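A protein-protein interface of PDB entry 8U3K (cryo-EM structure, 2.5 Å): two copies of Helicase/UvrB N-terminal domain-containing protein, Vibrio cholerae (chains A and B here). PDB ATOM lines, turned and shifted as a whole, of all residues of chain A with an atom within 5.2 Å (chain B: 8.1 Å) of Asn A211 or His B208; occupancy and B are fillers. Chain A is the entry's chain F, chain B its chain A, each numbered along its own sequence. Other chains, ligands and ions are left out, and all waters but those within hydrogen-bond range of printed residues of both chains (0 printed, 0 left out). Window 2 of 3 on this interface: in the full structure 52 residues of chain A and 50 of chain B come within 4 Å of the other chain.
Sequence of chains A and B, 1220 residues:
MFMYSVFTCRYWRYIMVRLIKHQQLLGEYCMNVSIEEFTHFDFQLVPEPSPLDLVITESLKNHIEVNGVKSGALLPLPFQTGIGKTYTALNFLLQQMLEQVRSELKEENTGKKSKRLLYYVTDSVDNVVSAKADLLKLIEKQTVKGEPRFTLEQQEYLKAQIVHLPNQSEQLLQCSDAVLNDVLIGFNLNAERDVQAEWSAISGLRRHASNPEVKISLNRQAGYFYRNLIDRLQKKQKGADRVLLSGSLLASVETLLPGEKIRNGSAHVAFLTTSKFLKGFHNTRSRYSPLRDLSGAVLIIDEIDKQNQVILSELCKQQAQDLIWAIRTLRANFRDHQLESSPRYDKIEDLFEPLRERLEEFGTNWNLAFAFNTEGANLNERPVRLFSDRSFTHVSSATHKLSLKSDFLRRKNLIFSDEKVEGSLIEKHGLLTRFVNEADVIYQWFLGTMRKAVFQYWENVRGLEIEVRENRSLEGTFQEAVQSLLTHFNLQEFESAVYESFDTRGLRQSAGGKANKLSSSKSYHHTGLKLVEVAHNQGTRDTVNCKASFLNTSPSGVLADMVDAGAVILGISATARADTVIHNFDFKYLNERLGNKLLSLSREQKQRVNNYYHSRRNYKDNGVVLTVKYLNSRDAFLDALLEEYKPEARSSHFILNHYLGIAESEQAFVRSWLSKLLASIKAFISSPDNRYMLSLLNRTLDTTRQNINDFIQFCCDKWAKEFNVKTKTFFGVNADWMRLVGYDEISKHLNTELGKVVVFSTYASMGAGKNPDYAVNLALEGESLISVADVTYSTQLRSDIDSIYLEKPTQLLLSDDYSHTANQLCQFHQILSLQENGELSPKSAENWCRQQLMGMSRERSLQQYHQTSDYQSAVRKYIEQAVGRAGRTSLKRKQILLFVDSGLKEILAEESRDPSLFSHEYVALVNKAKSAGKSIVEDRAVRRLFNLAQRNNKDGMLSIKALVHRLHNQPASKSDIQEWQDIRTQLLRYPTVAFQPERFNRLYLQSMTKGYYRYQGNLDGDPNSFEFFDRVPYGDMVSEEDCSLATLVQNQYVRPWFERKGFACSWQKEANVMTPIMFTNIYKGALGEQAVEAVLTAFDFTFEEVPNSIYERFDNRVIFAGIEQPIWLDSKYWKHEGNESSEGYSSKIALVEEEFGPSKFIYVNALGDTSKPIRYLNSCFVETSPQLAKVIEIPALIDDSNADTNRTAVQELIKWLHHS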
ATOM      1  N   HIS A 208       3.721 -12.379 -19.825  1.00  0.00           N
ATOM      2  CA  HIS A 208       4.390 -11.327 -20.580  1.00  0.00           C
ATOM      3  C   HIS A 208       3.488 -10.759 -21.669  1.00  0.00           C
ATOM      4  O   HIS A 208       3.225  -9.552 -21.674  1.00  0.00           O
ATOM      5  CB  HIS A 208       5.728 -11.820 -21.147  1.00  0.00           C
ATOM      6  CG  HIS A 208       5.636 -13.057 -21.983  1.00  0.00           C
ATOM      7  ND1 HIS A 208       5.311 -14.289 -21.459  1.00  0.00           N
ATOM      8  CD2 HIS A 208       5.863 -13.258 -23.303  1.00  0.00           C
ATOM      9  CE1 HIS A 208       5.327 -15.192 -22.421  1.00  0.00           C
ATOM     10  NE2 HIS A 208       5.660 -14.593 -23.549  1.00  0.00           N
ATOM     11  N   ALA A 209       3.001 -11.609 -22.577  1.00  0.00           N
ATOM     12  CA  ALA A 209       1.980 -11.254 -23.571  1.00  0.00           C
ATOM     13  C   ALA A 209       2.342 -10.018 -24.397  1.00  0.00           C
ATOM     14  O   ALA A 209       1.456  -9.313 -24.887  1.00  0.00           O
ATOM     15  CB  ALA A 209       0.612 -11.058 -22.910  1.00  0.00           C
ATOM     16  N   SER A 210       3.635  -9.732 -24.557  1.00  0.00           N
ATOM     17  CA  SER A 210       4.035  -8.530 -25.280  1.00  0.00           C
ATOM     18  C   SER A 210       3.898  -8.715 -26.786  1.00  0.00           C
ATOM     19  O   SER A 210       3.507  -7.785 -27.499  1.00  0.00           O
ATOM     20  CB  SER A 210       5.468  -8.157 -24.913  1.00  0.00           C
ATOM     21  OG  SER A 210       5.645  -8.160 -23.508  1.00  0.00           O
ATOM     22  N   ASN A 211       4.218  -9.894 -27.282  1.00  0.00           N
ATOM     23  CA  ASN A 211       4.225 -10.150 -28.712  1.00  0.00           C
ATOM     24  C   ASN A 211       2.795 -10.236 -29.246  1.00  0.00           C
ATOM     25  O   ASN A 211       1.916 -10.787 -28.578  1.00  0.00           O
ATOM     26  CB  ASN A 211       4.982 -11.440 -29.008  1.00  0.00           C
ATOM     27  CG  ASN A 211       4.627 -12.033 -30.348  1.00  0.00           C
ATOM     28  OD1 ASN A 211       3.794 -12.929 -30.437  1.00  0.00           O
ATOM     29  ND2 ASN A 211       5.267 -11.543 -31.401  1.00  0.00           N
ATOM     30  N   PRO A 212       2.533  -9.674 -30.430  1.00  0.00           N
ATOM     31  CA  PRO A 212       1.167  -9.716 -30.981  1.00  0.00           C
ATOM     32  C   PRO A 212       0.624 -11.116 -31.220  1.00  0.00           C
ATOM     33  O   PRO A 212      -0.564 -11.361 -30.977  1.00  0.00           O
ATOM     34  CB  PRO A 212       1.313  -8.940 -32.296  1.00  0.00           C
ATOM     35  CG  PRO A 212       2.449  -8.018 -32.052  1.00  0.00           C
ATOM     36  CD  PRO A 212       3.413  -8.789 -31.208  1.00  0.00           C
ATOM     37  N   GLU A 213       1.453 -12.044 -31.703  1.00  0.00           N
ATOM     38  CA  GLU A 213       0.966 -13.401 -31.928  1.00  0.00           C
ATOM     39  C   GLU A 213       0.689 -14.104 -30.611  1.00  0.00           C
ATOM     40  O   GLU A 213      -0.247 -14.910 -30.516  1.00  0.00           O
ATOM     41  CB  GLU A 213       1.968 -14.194 -32.759  1.00  0.00           C
ATOM     42  CG  GLU A 213       2.145 -13.675 -34.173  1.00  0.00           C
ATOM     43  CD  GLU A 213       3.145 -12.544 -34.256  1.00  0.00           C
ATOM     44  OE1 GLU A 213       3.981 -12.424 -33.338  1.00  0.00           O
ATOM     45  OE2 GLU A 213       3.098 -11.777 -35.240  1.00  0.00           O
ATOM     46  N   VAL A 214       1.488 -13.802 -29.588  1.00  0.00           N
ATOM     47  CA  VAL A 214       1.171 -14.240 -28.237  1.00  0.00           C
ATOM     48  C   VAL A 214      -0.193 -13.714 -27.823  1.00  0.00           C
ATOM     49  O   VAL A 214      -0.993 -14.433 -27.214  1.00  0.00           O
ATOM     50  CB  VAL A 214       2.273 -13.789 -27.265  1.00  0.00           C
ATOM     51  CG1 VAL A 214       1.861 -14.052 -25.847  1.00  0.00           C
ATOM     52  CG2 VAL A 214       3.553 -14.515 -27.569  1.00  0.00           C
ATOM     53  N   LYS A 215      -0.486 -12.457 -28.160  1.00  0.00           N
ATOM     54  CA  LYS A 215      -1.780 -11.877 -27.823  1.00  0.00           C
ATOM     55  C   LYS A 215      -2.911 -12.606 -28.538  1.00  0.00           C
ATOM     56  O   LYS A 215      -3.968 -12.854 -27.953  1.00  0.00           O
ATOM     57  CB  LYS A 215      -1.790 -10.389 -28.163  1.00  0.00           C
ATOM     58  CG  LYS A 215      -3.015  -9.656 -27.665  1.00  0.00           C
ATOM     59  CD  LYS A 215      -2.845  -9.230 -26.219  1.00  0.00           C
ATOM     60  CE  LYS A 215      -4.065  -9.602 -25.391  1.00  0.00           C
ATOM     61  NZ  LYS A 215      -4.267 -11.078 -25.355  1.00  0.00           N
ATOM     62  N   SER B 200       0.426 -17.326 -39.617  1.00  0.00           N
ATOM     63  CA  SER B 200       1.231 -16.211 -39.145  1.00  0.00           C
ATOM     64  C   SER B 200       1.306 -16.195 -37.627  1.00  0.00           C
ATOM     65  O   SER B 200       2.376 -15.956 -37.054  1.00  0.00           O
ATOM     66  CB  SER B 200       0.655 -14.899 -39.670  1.00  0.00           C
ATOM     67  OG  SER B 200       0.569 -14.924 -41.083  1.00  0.00           O
ATOM     68  N   ALA B 201       0.180 -16.459 -36.959  1.00  0.00           N
ATOM     69  CA  ALA B 201       0.187 -16.518 -35.500  1.00  0.00           C
ATOM     70  C   ALA B 201       1.099 -17.627 -34.998  1.00  0.00           C
ATOM     71  O   ALA B 201       1.872 -17.431 -34.048  1.00  0.00           O
ATOM     72  CB  ALA B 201      -1.233 -16.720 -34.978  1.00  0.00           C
ATOM     73  N   ILE B 202       1.034 -18.794 -35.635  1.00  0.00           N
ATOM     74  CA  ILE B 202       1.843 -19.929 -35.209  1.00  0.00           C
ATOM     75  C   ILE B 202       3.319 -19.646 -35.434  1.00  0.00           C
ATOM     76  O   ILE B 202       4.157 -19.950 -34.580  1.00  0.00           O
ATOM     77  CB  ILE B 202       1.383 -21.207 -35.929  1.00  0.00           C
ATOM     78  CG1 ILE B 202       0.225 -21.830 -35.167  1.00  0.00           C
ATOM     79  CG2 ILE B 202       2.507 -22.208 -36.054  1.00  0.00           C
ATOM     80  CD1 ILE B 202      -0.427 -22.929 -35.903  1.00  0.00           C
ATOM     81  N   SER B 203       3.658 -19.038 -36.572  1.00  0.00           N
ATOM     82  CA  SER B 203       5.045 -18.662 -36.818  1.00  0.00           C
ATOM     83  C   SER B 203       5.540 -17.679 -35.771  1.00  0.00           C
ATOM     84  O   SER B 203       6.611 -17.875 -35.184  1.00  0.00           O
ATOM     85  CB  SER B 203       5.184 -18.060 -38.211  1.00  0.00           C
ATOM     86  OG  SER B 203       5.036 -19.049 -39.205  1.00  0.00           O
ATOM     87  N   GLY B 204       4.747 -16.644 -35.488  1.00  0.00           N
ATOM     88  CA  GLY B 204       5.164 -15.648 -34.520  1.00  0.00           C
ATOM     89  C   GLY B 204       5.368 -16.228 -33.137  1.00  0.00           C
ATOM     90  O   GLY B 204       6.283 -15.826 -32.416  1.00  0.00           O
ATOM     91  N   LEU B 205       4.522 -17.180 -32.749  1.00  0.00           N
ATOM     92  CA  LEU B 205       4.780 -17.925 -31.522  1.00  0.00           C
ATOM     93  C   LEU B 205       6.068 -18.729 -31.635  1.00  0.00           C
ATOM     94  O   LEU B 205       6.854 -18.808 -30.685  1.00  0.00           O
ATOM     95  CB  LEU B 205       3.609 -18.847 -31.211  1.00  0.00           C
ATOM     96  CG  LEU B 205       2.479 -18.242 -30.394  1.00  0.00           C
ATOM     97  CD1 LEU B 205       1.299 -19.184 -30.372  1.00  0.00           C
ATOM     98  CD2 LEU B 205       2.958 -17.946 -28.998  1.00  0.00           C
ATOM     99  N   ARG B 206       6.304 -19.323 -32.806  1.00  0.00           N
ATOM    100  CA  ARG B 206       7.413 -20.251 -32.970  1.00  0.00           C
ATOM    101  C   ARG B 206       8.757 -19.549 -32.858  1.00  0.00           C
ATOM    102  O   ARG B 206       9.755 -20.173 -32.481  1.00  0.00           O
ATOM    103  CB  ARG B 206       7.292 -20.963 -34.316  1.00  0.00           C
ATOM    104  CG  ARG B 206       8.137 -22.205 -34.433  1.00  0.00           C
ATOM    105  CD  ARG B 206       8.562 -22.448 -35.862  1.00  0.00           C
ATOM    106  NE  ARG B 206       7.485 -22.972 -36.688  1.00  0.00           N
ATOM    107  CZ  ARG B 206       7.682 -23.751 -37.744  1.00  0.00           C
ATOM    108  NH1 ARG B 206       6.655 -24.192 -38.448  1.00  0.00           N
ATOM    109  NH2 ARG B 206       8.910 -24.096 -38.092  1.00  0.00           N
ATOM    110  N   ARG B 207       8.813 -18.255 -33.193  1.00  0.00           N
ATOM    111  CA  ARG B 207      10.078 -17.530 -33.052  1.00  0.00           C
ATOM    112  C   ARG B 207      10.610 -17.511 -31.626  1.00  0.00           C
ATOM    113  O   ARG B 207      11.829 -17.563 -31.436  1.00  0.00           O
ATOM    114  CB  ARG B 207       9.982 -16.077 -33.550  1.00  0.00           C
ATOM    115  CG  ARG B 207       9.095 -15.763 -34.755  1.00  0.00           C
ATOM    116  CD  ARG B 207       9.295 -16.696 -35.955  1.00  0.00           C
ATOM    117  NE  ARG B 207      10.671 -17.145 -36.138  1.00  0.00           N
ATOM    118  CZ  ARG B 207      11.391 -16.902 -37.224  1.00  0.00           C
ATOM    119  NH1 ARG B 207      12.637 -17.345 -37.310  1.00  0.00           N
ATOM    120  NH2 ARG B 207      10.859 -16.224 -38.230  1.00  0.00           N
ATOM    121  N   HIS B 208       9.748 -17.430 -30.621  1.00  0.00           N
ATOM    122  CA  HIS B 208      10.227 -17.348 -29.245  1.00  0.00           C
ATOM    123  C   HIS B 208       9.442 -18.303 -28.346  1.00  0.00           C
ATOM    124  O   HIS B 208       8.919 -17.928 -27.297  1.00  0.00           O
ATOM    125  CB  HIS B 208      10.199 -15.903 -28.749  1.00  0.00           C
ATOM    126  CG  HIS B 208       8.829 -15.324 -28.620  1.00  0.00           C
ATOM    127  ND1 HIS B 208       8.143 -15.306 -27.426  1.00  0.00           N
ATOM    128  CD2 HIS B 208       8.022 -14.731 -29.530  1.00  0.00           C
ATOM    129  CE1 HIS B 208       6.971 -14.726 -27.607  1.00  0.00           C
ATOM    130  NE2 HIS B 208       6.872 -14.370 -28.875  1.00  0.00           N
ATOM    131  N   ALA B 209       9.373 -19.572 -28.750  1.00  0.00           N
ATOM    132  CA  ALA B 209       8.660 -20.592 -27.989  1.00  0.00           C
ATOM    133  C   ALA B 209       9.465 -21.154 -26.824  1.00  0.00           C
ATOM    134  O   ALA B 209       9.179 -22.272 -26.387  1.00  0.00           O
ATOM    135  CB  ALA B 209       8.248 -21.738 -28.912  1.00  0.00           C
ATOM    136  N   SER B 210      10.467 -20.425 -26.327  1.00  0.00           N
ATOM    137  CA  SER B 210      11.284 -20.931 -25.228  1.00  0.00           C
ATOM    138  C   SER B 210      10.469 -21.099 -23.950  1.00  0.00           C
ATOM    139  O   SER B 210      10.715 -22.022 -23.166  1.00  0.00           O
ATOM    140  CB  SER B 210      12.467 -19.997 -24.987  1.00  0.00           C
ATOM    141  OG  SER B 210      13.291 -20.489 -23.946  1.00  0.00           O
ATOM    142  N   ASN B 211       9.513 -20.210 -23.715  1.00  0.00           N
ATOM    143  CA  ASN B 211       8.687 -20.301 -22.521  1.00  0.00           C
ATOM    144  C   ASN B 211       7.810 -21.551 -22.573  1.00  0.00           C
ATOM    145  O   ASN B 211       7.332 -21.929 -23.645  1.00  0.00           O
ATOM    146  CB  ASN B 211       7.810 -19.060 -22.391  1.00  0.00           C
ATOM    147  CG  ASN B 211       6.905 -19.109 -21.183  1.00  0.00           C
ATOM    148  OD1 ASN B 211       5.692 -19.260 -21.316  1.00  0.00           O
ATOM    149  ND2 ASN B 211       7.482 -18.960 -19.999  1.00  0.00           N
ATOM    150  N   PRO B 212       7.602 -22.224 -21.438  1.00  0.00           N
ATOM    151  CA  PRO B 212       6.730 -23.410 -21.434  1.00  0.00           C
ATOM    152  C   PRO B 212       5.286 -23.133 -21.823  1.00  0.00           C
ATOM    153  O   PRO B 212       4.778 -23.779 -22.745  1.00  0.00           O
ATOM    154  CB  PRO B 212       6.839 -23.902 -19.989  1.00  0.00           C
ATOM    155  CG  PRO B 212       8.182 -23.463 -19.563  1.00  0.00           C
ATOM    156  CD  PRO B 212       8.383 -22.119 -20.196  1.00  0.00           C
ATOM    157  N   VAL B 214       3.994 -20.846 -23.477  1.00  0.00           N
ATOM    158  CA  VAL B 214       4.046 -20.663 -24.916  1.00  0.00           C
ATOM    159  C   VAL B 214       4.090 -22.011 -25.621  1.00  0.00           C
ATOM    160  O   VAL B 214       3.477 -22.186 -26.675  1.00  0.00           O
ATOM    161  CB  VAL B 214       5.243 -19.774 -25.291  1.00  0.00           C
ATOM    162  CG1 VAL B 214       5.357 -19.641 -26.786  1.00  0.00           C
ATOM    163  CG2 VAL B 214       5.088 -18.411 -24.664  1.00  0.00           C
ATOM    164  N   LYS B 215       4.781 -22.998 -25.041  1.00  0.00           N
ATOM    165  CA  LYS B 215       4.900 -24.285 -25.719  1.00  0.00           C
ATOM    166  C   LYS B 215       3.577 -25.044 -25.727  1.00  0.00           C
ATOM    167  O   LYS B 215       3.210 -25.628 -26.750  1.00  0.00           O
ATOM    168  CB  LYS B 215       6.012 -25.136 -25.102  1.00  0.00           C
ATOM    169  CG  LYS B 215       7.398 -24.864 -25.662  1.00  0.00           C
ATOM    170  CD  LYS B 215       7.608 -25.430 -27.068  1.00  0.00           C
ATOM    171  CE  LYS B 215       6.882 -26.752 -27.296  1.00  0.00           C
ATOM    172  NZ  LYS B 215       6.753 -27.072 -28.740  1.00  0.00           N
ATOM    173  N   LEU B 218       1.351 -23.190 -28.235  1.00  0.00           N
ATOM    174  CA  LEU B 218       1.820 -23.443 -29.586  1.00  0.00           C
ATOM    175  C   LEU B 218       1.496 -24.860 -30.020  1.00  0.00           C
ATOM    176  O   LEU B 218       1.132 -25.087 -31.175  1.00  0.00           O
ATOM    177  CB  LEU B 218       3.320 -23.179 -29.666  1.00  0.00           C
ATOM    178  CG  LEU B 218       3.998 -23.443 -31.003  1.00  0.00           C
ATOM    179  CD1 LEU B 218       3.287 -22.708 -32.110  1.00  0.00           C
ATOM    180  CD2 LEU B 218       5.441 -23.022 -30.935  1.00  0.00           C
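His A208 touches Val B214, and with the chains exchanged Val A214 touches His B208. Asn A211 touches His B208, but with the chains exchanged His A208 does not touch Asn B211 (4.2 Å). Positions printed for both chains: 208, 209, 210, 211, 212, 214 and 215.
Asn A211 touches just one residue of chain B: His B208. His B208 touches two residues of chain A. No residue of chain B comes within 4 Å of Pro A212. Printed residues of chain B within 4 Å of Glu A213: Ser B200, Ala B201, Gly B204 and Leu B205. Of the printed residues of chain A, Val B214 touches His A208 (3.9 Å). Of the printed residues of chain A, Leu B205 touches Glu A213 (3.9 Å) and Val A214 (3.8 Å). Arg B206 touches none of the printed residues of chain A. Lys A215 touches none of the printed residues of chain B. The nearest residue of chain B that does not touch Asn A211 is Gly B204 (4.3 Å). The nearest residue of chain A that does not touch His B208 is His A208 (4.3 Å). The nearest printed residue of chain B that does not touch Val A214 is Val B214 (5.1 Å).
OD1 of Asn B211 sits at hydrogen-bond distance from N of Val B214, 3.2 Å away. The side-chain hydroxyl (OG) of Ser A210 sits at hydrogen-bond distance from the backbone carbonyl oxygen (O) of His A208 (3.3 Å). The side-chain amide nitrogen of Asn A211 sits at hydrogen-bond distance from the side-chain carboxylate of Glu A213. The side-chain amide oxygen (OD1) of Asn A211 lies within hydrogen-bond range of the backbone NH (N) of Val A214.
Of the 8 printed residues of chain A, 4 touch a printed residue of chain B. Printed residues of chain A that touch a printed residue of chain B: His A208, Asn A211, Glu A213 and Val A214. Of the 16 printed residues of chain B, 6 touch a printed residue of chain A. Hydrophobic or aromatic side chains of chain B that line the printed part of chain A: Leu B205, His B208 and Val B214. Among the printed residues, 8 pairs touch across the chains. Among the printed residues, no Asp or Glu carboxylate lies within 4 Å of a Lys or Arg side-chain nitrogen of the other chain.
His A208 touches Val B214 (CE1 to CG2, 3.9 Å). NE2 of His B208 touches CB of Asn A211 (3.5 Å). Glu A213 touches Ser B200. Glu A213 touches Ala B201 (CB to O, 3.5 Å). Glu A213 touches Gly B204. Glu A213 touches Leu B205 (CB to N, 3.9 Å). Val A214 touches Leu B205. Val A214 touches His B208.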
